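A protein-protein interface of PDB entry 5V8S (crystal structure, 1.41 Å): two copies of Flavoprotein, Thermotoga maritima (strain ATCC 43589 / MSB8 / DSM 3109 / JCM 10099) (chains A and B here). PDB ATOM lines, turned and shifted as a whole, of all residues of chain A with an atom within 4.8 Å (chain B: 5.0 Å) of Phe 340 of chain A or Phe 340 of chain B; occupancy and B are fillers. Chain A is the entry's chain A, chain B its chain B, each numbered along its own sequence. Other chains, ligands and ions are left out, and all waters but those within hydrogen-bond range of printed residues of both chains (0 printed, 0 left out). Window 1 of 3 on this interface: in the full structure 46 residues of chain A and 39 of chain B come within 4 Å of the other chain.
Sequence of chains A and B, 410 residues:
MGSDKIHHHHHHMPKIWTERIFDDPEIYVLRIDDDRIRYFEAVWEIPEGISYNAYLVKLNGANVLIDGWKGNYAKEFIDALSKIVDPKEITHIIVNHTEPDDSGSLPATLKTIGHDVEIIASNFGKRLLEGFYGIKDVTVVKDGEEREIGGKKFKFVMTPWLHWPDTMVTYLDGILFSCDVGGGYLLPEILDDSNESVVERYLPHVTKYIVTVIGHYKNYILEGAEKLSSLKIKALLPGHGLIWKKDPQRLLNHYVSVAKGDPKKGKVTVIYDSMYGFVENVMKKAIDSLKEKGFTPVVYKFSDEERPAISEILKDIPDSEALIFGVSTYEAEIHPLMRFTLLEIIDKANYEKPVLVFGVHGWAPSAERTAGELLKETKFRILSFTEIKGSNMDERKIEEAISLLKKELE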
ATOM      1  N   VAL A  43      16.507  -9.806   7.845  1.00  0.00           N
ATOM      2  CA  VAL A  43      16.241  -8.531   7.183  1.00  0.00           C
ATOM      3  C   VAL A  43      15.096  -7.703   7.767  1.00  0.00           C
ATOM      4  O   VAL A  43      15.220  -6.475   7.833  1.00  0.00           O
ATOM      5  CB  VAL A  43      16.123  -8.683   5.653  1.00  0.00           C
ATOM      6  CG1 VAL A  43      15.155  -9.713   5.293  1.00  0.00           C
ATOM      7  CG2 VAL A  43      15.752  -7.350   4.968  1.00  0.00           C
ATOM      8  N   ILE A 310      12.196  -0.749   7.052  1.00  0.00           N
ATOM      9  CA  ILE A 310      11.591  -1.115   5.780  1.00  0.00           C
ATOM     10  C   ILE A 310      10.384  -2.034   5.997  1.00  0.00           C
ATOM     11  O   ILE A 310       9.424  -1.998   5.216  1.00  0.00           O
ATOM     12  CB  ILE A 310      12.656  -1.726   4.849  1.00  0.00           C
ATOM     13  CG1 ILE A 310      13.952  -0.893   4.888  1.00  0.00           C
ATOM     14  CG2 ILE A 310      12.117  -1.834   3.422  1.00  0.00           C
ATOM     15  CD1 ILE A 310      13.831   0.575   4.484  1.00  0.00           C
ATOM     16  N   PRO A 336      20.671   5.045  -2.466  1.00  0.00           N
ATOM     17  CA  PRO A 336      20.643   3.721  -1.859  1.00  0.00           C
ATOM     18  C   PRO A 336      19.458   3.297  -1.013  1.00  0.00           C
ATOM     19  O   PRO A 336      18.876   2.286  -1.354  1.00  0.00           O
ATOM     20  CB  PRO A 336      21.920   3.693  -1.018  1.00  0.00           C
ATOM     21  CG  PRO A 336      22.825   4.644  -1.700  1.00  0.00           C
ATOM     22  CD  PRO A 336      21.939   5.741  -2.196  1.00  0.00           C
ATOM     23  N   LEU A 337      18.923   4.176  -0.174  1.00  0.00           N
ATOM     24  CA  LEU A 337      17.807   3.750   0.661  1.00  0.00           C
ATOM     25  C   LEU A 337      16.496   3.760  -0.112  1.00  0.00           C
ATOM     26  O   LEU A 337      15.665   2.864   0.061  1.00  0.00           O
ATOM     27  CB  LEU A 337      17.708   4.608   1.914  1.00  0.00           C
ATOM     28  CG  LEU A 337      18.754   4.256   2.963  1.00  0.00           C
ATOM     29  CD1 LEU A 337      19.041   5.387   3.886  1.00  0.00           C
ATOM     30  CD2 LEU A 337      18.227   3.069   3.763  1.00  0.00           C
ATOM     31  N   MET A 338      16.283   4.758  -0.964  1.00  0.00           N
ATOM     32  CA  MET A 338      15.077   4.757  -1.785  1.00  0.00           C
ATOM     33  C   MET A 338      15.148   3.686  -2.873  1.00  0.00           C
ATOM     34  O   MET A 338      14.110   3.137  -3.266  1.00  0.00           O
ATOM     35  CB  MET A 338      14.785   6.156  -2.340  1.00  0.00           C
ATOM     36  CG  MET A 338      14.377   7.162  -1.259  1.00  0.00           C
ATOM     37  SD  MET A 338      12.748   6.911  -0.505  1.00  0.00           S
ATOM     38  CE  MET A 338      11.656   7.390  -1.840  1.00  0.00           C
ATOM     39  N   ARG A 339      16.353   3.331  -3.337  1.00  0.00           N
ATOM     40  CA  ARG A 339      16.458   2.173  -4.218  1.00  0.00           C
ATOM     41  C   ARG A 339      16.046   0.898  -3.485  1.00  0.00           C
ATOM     42  O   ARG A 339      15.220   0.121  -3.981  1.00  0.00           O
ATOM     43  CB  ARG A 339      17.877   2.026  -4.768  1.00  0.00           C
ATOM     44  CG  ARG A 339      17.983   0.900  -5.787  1.00  0.00           C
ATOM     45  CD  ARG A 339      19.427   0.530  -6.080  1.00  0.00           C
ATOM     46  NE  ARG A 339      20.091  -0.018  -4.905  1.00  0.00           N
ATOM     47  CZ  ARG A 339      21.196   0.465  -4.343  1.00  0.00           C
ATOM     48  NH1 ARG A 339      21.800   1.530  -4.841  1.00  0.00           N
ATOM     49  NH2 ARG A 339      21.697  -0.125  -3.272  1.00  0.00           N
ATOM     50  N   PHE A 340      16.613   0.672  -2.296  1.00  0.00           N
ATOM     51  CA  PHE A 340      16.285  -0.534  -1.540  1.00  0.00           C
ATOM     52  C   PHE A 340      14.789  -0.598  -1.274  1.00  0.00           C
ATOM     53  O   PHE A 340      14.162  -1.642  -1.452  1.00  0.00           O
ATOM     54  CB  PHE A 340      17.068  -0.549  -0.221  1.00  0.00           C
ATOM     55  CG  PHE A 340      16.854  -1.788   0.611  1.00  0.00           C
ATOM     56  CD1 PHE A 340      17.615  -2.918   0.398  1.00  0.00           C
ATOM     57  CD2 PHE A 340      15.892  -1.823   1.606  1.00  0.00           C
ATOM     58  CE1 PHE A 340      17.426  -4.056   1.159  1.00  0.00           C
ATOM     59  CE2 PHE A 340      15.709  -2.961   2.358  1.00  0.00           C
ATOM     60  CZ  PHE A 340      16.486  -4.070   2.143  1.00  0.00           C
ATOM     61  N   THR A 341      14.212   0.520  -0.843  1.00  0.00           N
ATOM     62  CA  THR A 341      12.787   0.565  -0.527  1.00  0.00           C
ATOM     63  C   THR A 341      11.942   0.259  -1.759  1.00  0.00           C
ATOM     64  O   THR A 341      11.020  -0.559  -1.696  1.00  0.00           O
ATOM     65  CB  THR A 341      12.436   1.928   0.060  1.00  0.00           C
ATOM     66  OG1 THR A 341      13.157   2.110   1.270  1.00  0.00           O
ATOM     67  CG2 THR A 341      10.911   2.032   0.375  1.00  0.00           C
ATOM     68  N   LEU A 342      12.242   0.914  -2.886  1.00  0.00           N
ATOM     69  CA  LEU A 342      11.487   0.675  -4.116  1.00  0.00           C
ATOM     70  C   LEU A 342      11.613  -0.772  -4.572  1.00  0.00           C
ATOM     71  O   LEU A 342      10.622  -1.392  -4.980  1.00  0.00           O
ATOM     72  CB  LEU A 342      11.966   1.615  -5.221  1.00  0.00           C
ATOM     73  CG  LEU A 342      11.606   3.086  -5.015  1.00  0.00           C
ATOM     74  CD1 LEU A 342      12.265   3.945  -6.073  1.00  0.00           C
ATOM     75  CD2 LEU A 342      10.111   3.306  -5.018  1.00  0.00           C
ATOM     76  N   LEU A 343      12.827  -1.329  -4.518  1.00  0.00           N
ATOM     77  CA  LEU A 343      12.985  -2.719  -4.939  1.00  0.00           C
ATOM     78  C   LEU A 343      12.210  -3.667  -4.036  1.00  0.00           C
ATOM     79  O   LEU A 343      11.639  -4.644  -4.517  1.00  0.00           O
ATOM     80  CB  LEU A 343      14.459  -3.117  -4.985  1.00  0.00           C
ATOM     81  CG  LEU A 343      15.297  -2.471  -6.084  1.00  0.00           C
ATOM     82  CD1 LEU A 343      16.774  -2.851  -5.940  1.00  0.00           C
ATOM     83  CD2 LEU A 343      14.803  -2.890  -7.442  1.00  0.00           C
ATOM     84  N   GLU A 344      12.174  -3.399  -2.724  1.00  0.00           N
ATOM     85  CA  GLU A 344      11.397  -4.263  -1.842  1.00  0.00           C
ATOM     86  C   GLU A 344       9.897  -4.071  -2.018  1.00  0.00           C
ATOM     87  O   GLU A 344       9.145  -5.043  -1.872  1.00  0.00           O
ATOM     88  CB  GLU A 344      11.807  -4.091  -0.385  1.00  0.00           C
ATOM     89  CG  GLU A 344      13.248  -4.512  -0.111  1.00  0.00           C
ATOM     90  CD  GLU A 344      13.556  -5.885  -0.608  1.00  0.00           C
ATOM     91  OE1 GLU A 344      12.726  -6.797  -0.415  1.00  0.00           O
ATOM     92  OE2 GLU A 344      14.638  -6.054  -1.199  1.00  0.00           O
ATOM     93  N   ILE B 310      26.740  -0.069   6.466  1.00  0.00           N
ATOM     94  CA  ILE B 310      27.340  -0.128   5.133  1.00  0.00           C
ATOM     95  C   ILE B 310      28.559   0.786   5.040  1.00  0.00           C
ATOM     96  O   ILE B 310      29.523   0.484   4.324  1.00  0.00           O
ATOM     97  CB  ILE B 310      26.307   0.160   4.023  1.00  0.00           C
ATOM     98  CG1 ILE B 310      26.920  -0.056   2.631  1.00  0.00           C
ATOM     99  CG2 ILE B 310      25.766   1.601   4.130  1.00  0.00           C
ATOM    100  CD1 ILE B 310      27.391  -1.477   2.318  1.00  0.00           C
ATOM    101  N   PRO B 336      18.344  -9.769   0.329  1.00  0.00           N
ATOM    102  CA  PRO B 336      18.276  -8.328   0.059  1.00  0.00           C
ATOM    103  C   PRO B 336      19.440  -7.534   0.608  1.00  0.00           C
ATOM    104  O   PRO B 336      19.828  -6.538  -0.007  1.00  0.00           O
ATOM    105  CB  PRO B 336      16.961  -7.925   0.734  1.00  0.00           C
ATOM    106  CG  PRO B 336      16.163  -9.103   0.705  1.00  0.00           C
ATOM    107  CD  PRO B 336      17.062 -10.277   0.851  1.00  0.00           C
ATOM    108  N   LEU B 337      19.978  -7.899   1.769  1.00  0.00           N
ATOM    109  CA  LEU B 337      21.040  -7.078   2.334  1.00  0.00           C
ATOM    110  C   LEU B 337      22.372  -7.337   1.651  1.00  0.00           C
ATOM    111  O   LEU B 337      23.213  -6.437   1.599  1.00  0.00           O
ATOM    112  CB  LEU B 337      21.120  -7.252   3.862  1.00  0.00           C
ATOM    113  CG  LEU B 337      19.898  -6.676   4.592  1.00  0.00           C
ATOM    114  CD1 LEU B 337      20.058  -6.851   6.067  1.00  0.00           C
ATOM    115  CD2 LEU B 337      19.658  -5.220   4.288  1.00  0.00           C
ATOM    116  N   MET B 338      22.573  -8.534   1.108  1.00  0.00           N
ATOM    117  CA  MET B 338      23.755  -8.777   0.284  1.00  0.00           C
ATOM    118  C   MET B 338      23.620  -8.131  -1.096  1.00  0.00           C
ATOM    119  O   MET B 338      24.616  -7.645  -1.649  1.00  0.00           O
ATOM    120  CB  MET B 338      24.028 -10.287   0.188  1.00  0.00           C
ATOM    121  CG  MET B 338      24.531 -10.885   1.504  1.00  0.00           C
ATOM    122  SD  MET B 338      26.036 -10.144   2.162  1.00  0.00           S
ATOM    123  CE  MET B 338      27.254 -10.739   0.975  1.00  0.00           C
ATOM    124  N   ARG B 339      22.404  -8.072  -1.650  1.00  0.00           N
ATOM    125  CA  ARG B 339      22.188  -7.279  -2.865  1.00  0.00           C
ATOM    126  C   ARG B 339      22.573  -5.826  -2.635  1.00  0.00           C
ATOM    127  O   ARG B 339      23.339  -5.243  -3.410  1.00  0.00           O
ATOM    128  CB  ARG B 339      20.727  -7.335  -3.313  1.00  0.00           C
ATOM    129  CG  ARG B 339      20.486  -6.614  -4.630  1.00  0.00           C
ATOM    130  CD  ARG B 339      19.022  -6.399  -4.893  1.00  0.00           C
ATOM    131  NE  ARG B 339      18.435  -5.465  -3.946  1.00  0.00           N
ATOM    132  CZ  ARG B 339      17.357  -5.688  -3.199  1.00  0.00           C
ATOM    133  NH1 ARG B 339      16.704  -6.843  -3.245  1.00  0.00           N
ATOM    134  NH2 ARG B 339      16.932  -4.724  -2.389  1.00  0.00           N
ATOM    135  N   PHE B 340      22.036  -5.232  -1.575  1.00  0.00           N
ATOM    136  CA  PHE B 340      22.317  -3.838  -1.259  1.00  0.00           C
ATOM    137  C   PHE B 340      23.816  -3.620  -1.110  1.00  0.00           C
ATOM    138  O   PHE B 340      24.378  -2.659  -1.652  1.00  0.00           O
ATOM    139  CB  PHE B 340      21.588  -3.482   0.037  1.00  0.00           C
ATOM    140  CG  PHE B 340      21.824  -2.065   0.494  1.00  0.00           C
ATOM    141  CD1 PHE B 340      21.043  -1.029   0.034  1.00  0.00           C
ATOM    142  CD2 PHE B 340      22.824  -1.783   1.390  1.00  0.00           C
ATOM    143  CE1 PHE B 340      21.264   0.288   0.454  1.00  0.00           C
ATOM    144  CE2 PHE B 340      23.049  -0.494   1.805  1.00  0.00           C
ATOM    145  CZ  PHE B 340      22.283   0.547   1.334  1.00  0.00           C
ATOM    146  N   THR B 341      24.471  -4.485  -0.344  1.00  0.00           N
ATOM    147  CA  THR B 341      25.894  -4.314  -0.075  1.00  0.00           C
ATOM    148  C   THR B 341      26.712  -4.432  -1.349  1.00  0.00           C
ATOM    149  O   THR B 341      27.630  -3.634  -1.582  1.00  0.00           O
ATOM    150  CB  THR B 341      26.337  -5.325   0.977  1.00  0.00           C
ATOM    151  OG1 THR B 341      25.663  -5.036   2.206  1.00  0.00           O
ATOM    152  CG2 THR B 341      27.825  -5.243   1.221  1.00  0.00           C
ATOM    153  N   LEU B 342      26.428  -5.442  -2.169  1.00  0.00           N
ATOM    154  CA  LEU B 342      27.159  -5.589  -3.427  1.00  0.00           C
ATOM    155  C   LEU B 342      26.932  -4.386  -4.327  1.00  0.00           C
ATOM    156  O   LEU B 342      27.866  -3.907  -4.970  1.00  0.00           O
ATOM    157  CB  LEU B 342      26.788  -6.899  -4.134  1.00  0.00           C
ATOM    158  CG  LEU B 342      27.320  -8.189  -3.516  1.00  0.00           C
ATOM    159  CD1 LEU B 342      26.525  -9.379  -4.067  1.00  0.00           C
ATOM    160  CD2 LEU B 342      28.786  -8.343  -3.806  1.00  0.00           C
ATOM    161  N   LEU B 343      25.700  -3.887  -4.397  1.00  0.00           N
ATOM    162  CA  LEU B 343      25.459  -2.735  -5.253  1.00  0.00           C
ATOM    163  C   LEU B 343      26.239  -1.517  -4.767  1.00  0.00           C
ATOM    164  O   LEU B 343      26.754  -0.744  -5.592  1.00  0.00           O
ATOM    165  CB  LEU B 343      23.964  -2.422  -5.353  1.00  0.00           C
ATOM    166  CG  LEU B 343      23.135  -3.403  -6.177  1.00  0.00           C
ATOM    167  CD1 LEU B 343      21.669  -3.052  -6.054  1.00  0.00           C
ATOM    168  CD2 LEU B 343      23.581  -3.411  -7.649  1.00  0.00           C
ATOM    169  N   GLU B 344      26.390  -1.345  -3.447  1.00  0.00           N
ATOM    170  CA  GLU B 344      27.146  -0.193  -2.957  1.00  0.00           C
ATOM    171  C   GLU B 344      28.639  -0.386  -3.162  1.00  0.00           C
ATOM    172  O   GLU B 344      29.345   0.576  -3.470  1.00  0.00           O
ATOM    173  CB  GLU B 344      26.826   0.096  -1.484  1.00  0.00           C
ATOM    174  CG  GLU B 344      25.384   0.559  -1.263  1.00  0.00           C
ATOM    175  CD  GLU B 344      25.031   1.676  -2.197  1.00  0.00           C
ATOM    176  OE1 GLU B 344      25.838   2.645  -2.281  1.00  0.00           O
ATOM    177  OE2 GLU B 344      23.996   1.582  -2.882  1.00  0.00           O
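The guanidinium group of Arg 339 of chain A lies within salt-bridge range of the side-chain carboxylate of Glu 344 of chain B (2.9 Å).
The side-chain carboxylate of Glu 344 of chain A lies within salt-bridge range of the guanidinium group of Arg 339 of chain B (2.9 Å).
The side-chain hydroxyl (OG1) of Thr 341 of chain B sits at hydrogen-bond distance from the backbone carbonyl oxygen (O) of Leu 337 of chain B, 2.9 Å away.
Among the printed residues, merely in contact across the chains: Phe 340 of chain A with Arg 339 of chain B (3.4 Å), Pro 336 of chain A with Glu 344 of chain B (3.5 Å), Arg 339 of chain A with Phe 340 of chain B (3.5 Å), Glu 344 of chain A with Pro 336 of chain B (3.6 Å), Pro 336 of chain A with Phe 340 of chain B (3.6 Å), Arg 339 of chain A with Leu 343 of chain B (3.6 Å), Phe 340 of chain A with Pro 336 of chain B (3.6 Å), Leu 343 of chain A with Arg 339 of chain B (3.7 Å), Phe 340 of chain A with Phe 340 of chain B (3.9 Å) and Phe 340 of chain A with Leu 337 of chain B (3.998 Å).
Of the printed residues of chain B, Pro 336 of chain A touches Phe 340 and Glu 344.
Printed residues of chain B within 4 Å of Arg 339 of chain A: Phe 340 (3.5 Å), Leu 343 (3.6 Å) and Glu 344 (2.9 Å).
Of the printed residues of chain B, Phe 340 of chain A touches Pro 336, Leu 337, Arg 339 and Phe 340.
Printed residues of chain A within 4 Å of Phe 340 of chain B: Pro 336, Arg 339 and Phe 340.
Thr 341 of chain B touches none of the printed residues of chain A.
The nearest printed residue of chain B that does not touch Leu 343 of chain A is Leu 343 of chain B (4.9 Å).
Of the 11 printed residues of chain A, 5 touch a printed residue of chain B.
Printed residues of chain A that touch a printed residue of chain B: Pro 336, Arg 339, Phe 340, Leu 343 and Glu 344.
Among the printed residues, 12 pairs touch across the chains.
Among the printed residues, Asp or Glu carboxylates within 4 Å of a Lys or Arg side-chain nitrogen of the other chain: Arg 339 of chain A with Glu 344 of chain B and Glu 344 of chain A with Arg 339 of chain B.
Pro 336 of chain A touches Phe 340 of chain B, and with the chains exchanged Phe 340 of chain A touches Pro 336 of chain B.
Pro 336 of chain A touches Glu 344 of chain B, and with the chains exchanged Glu 344 of chain A touches Pro 336 of chain B.
Arg 339 of chain A touches Glu 344 of chain B, and with the chains exchanged Glu 344 of chain A touches Arg 339 of chain B.
Phe 340 of chain B touches its own counterpart, Phe 340 of chain A.
10 positions are printed for both chains.
Of the 12 pairs that touch across the chains among the printed residues, 11 have their exchanged pair printed and touching as well.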
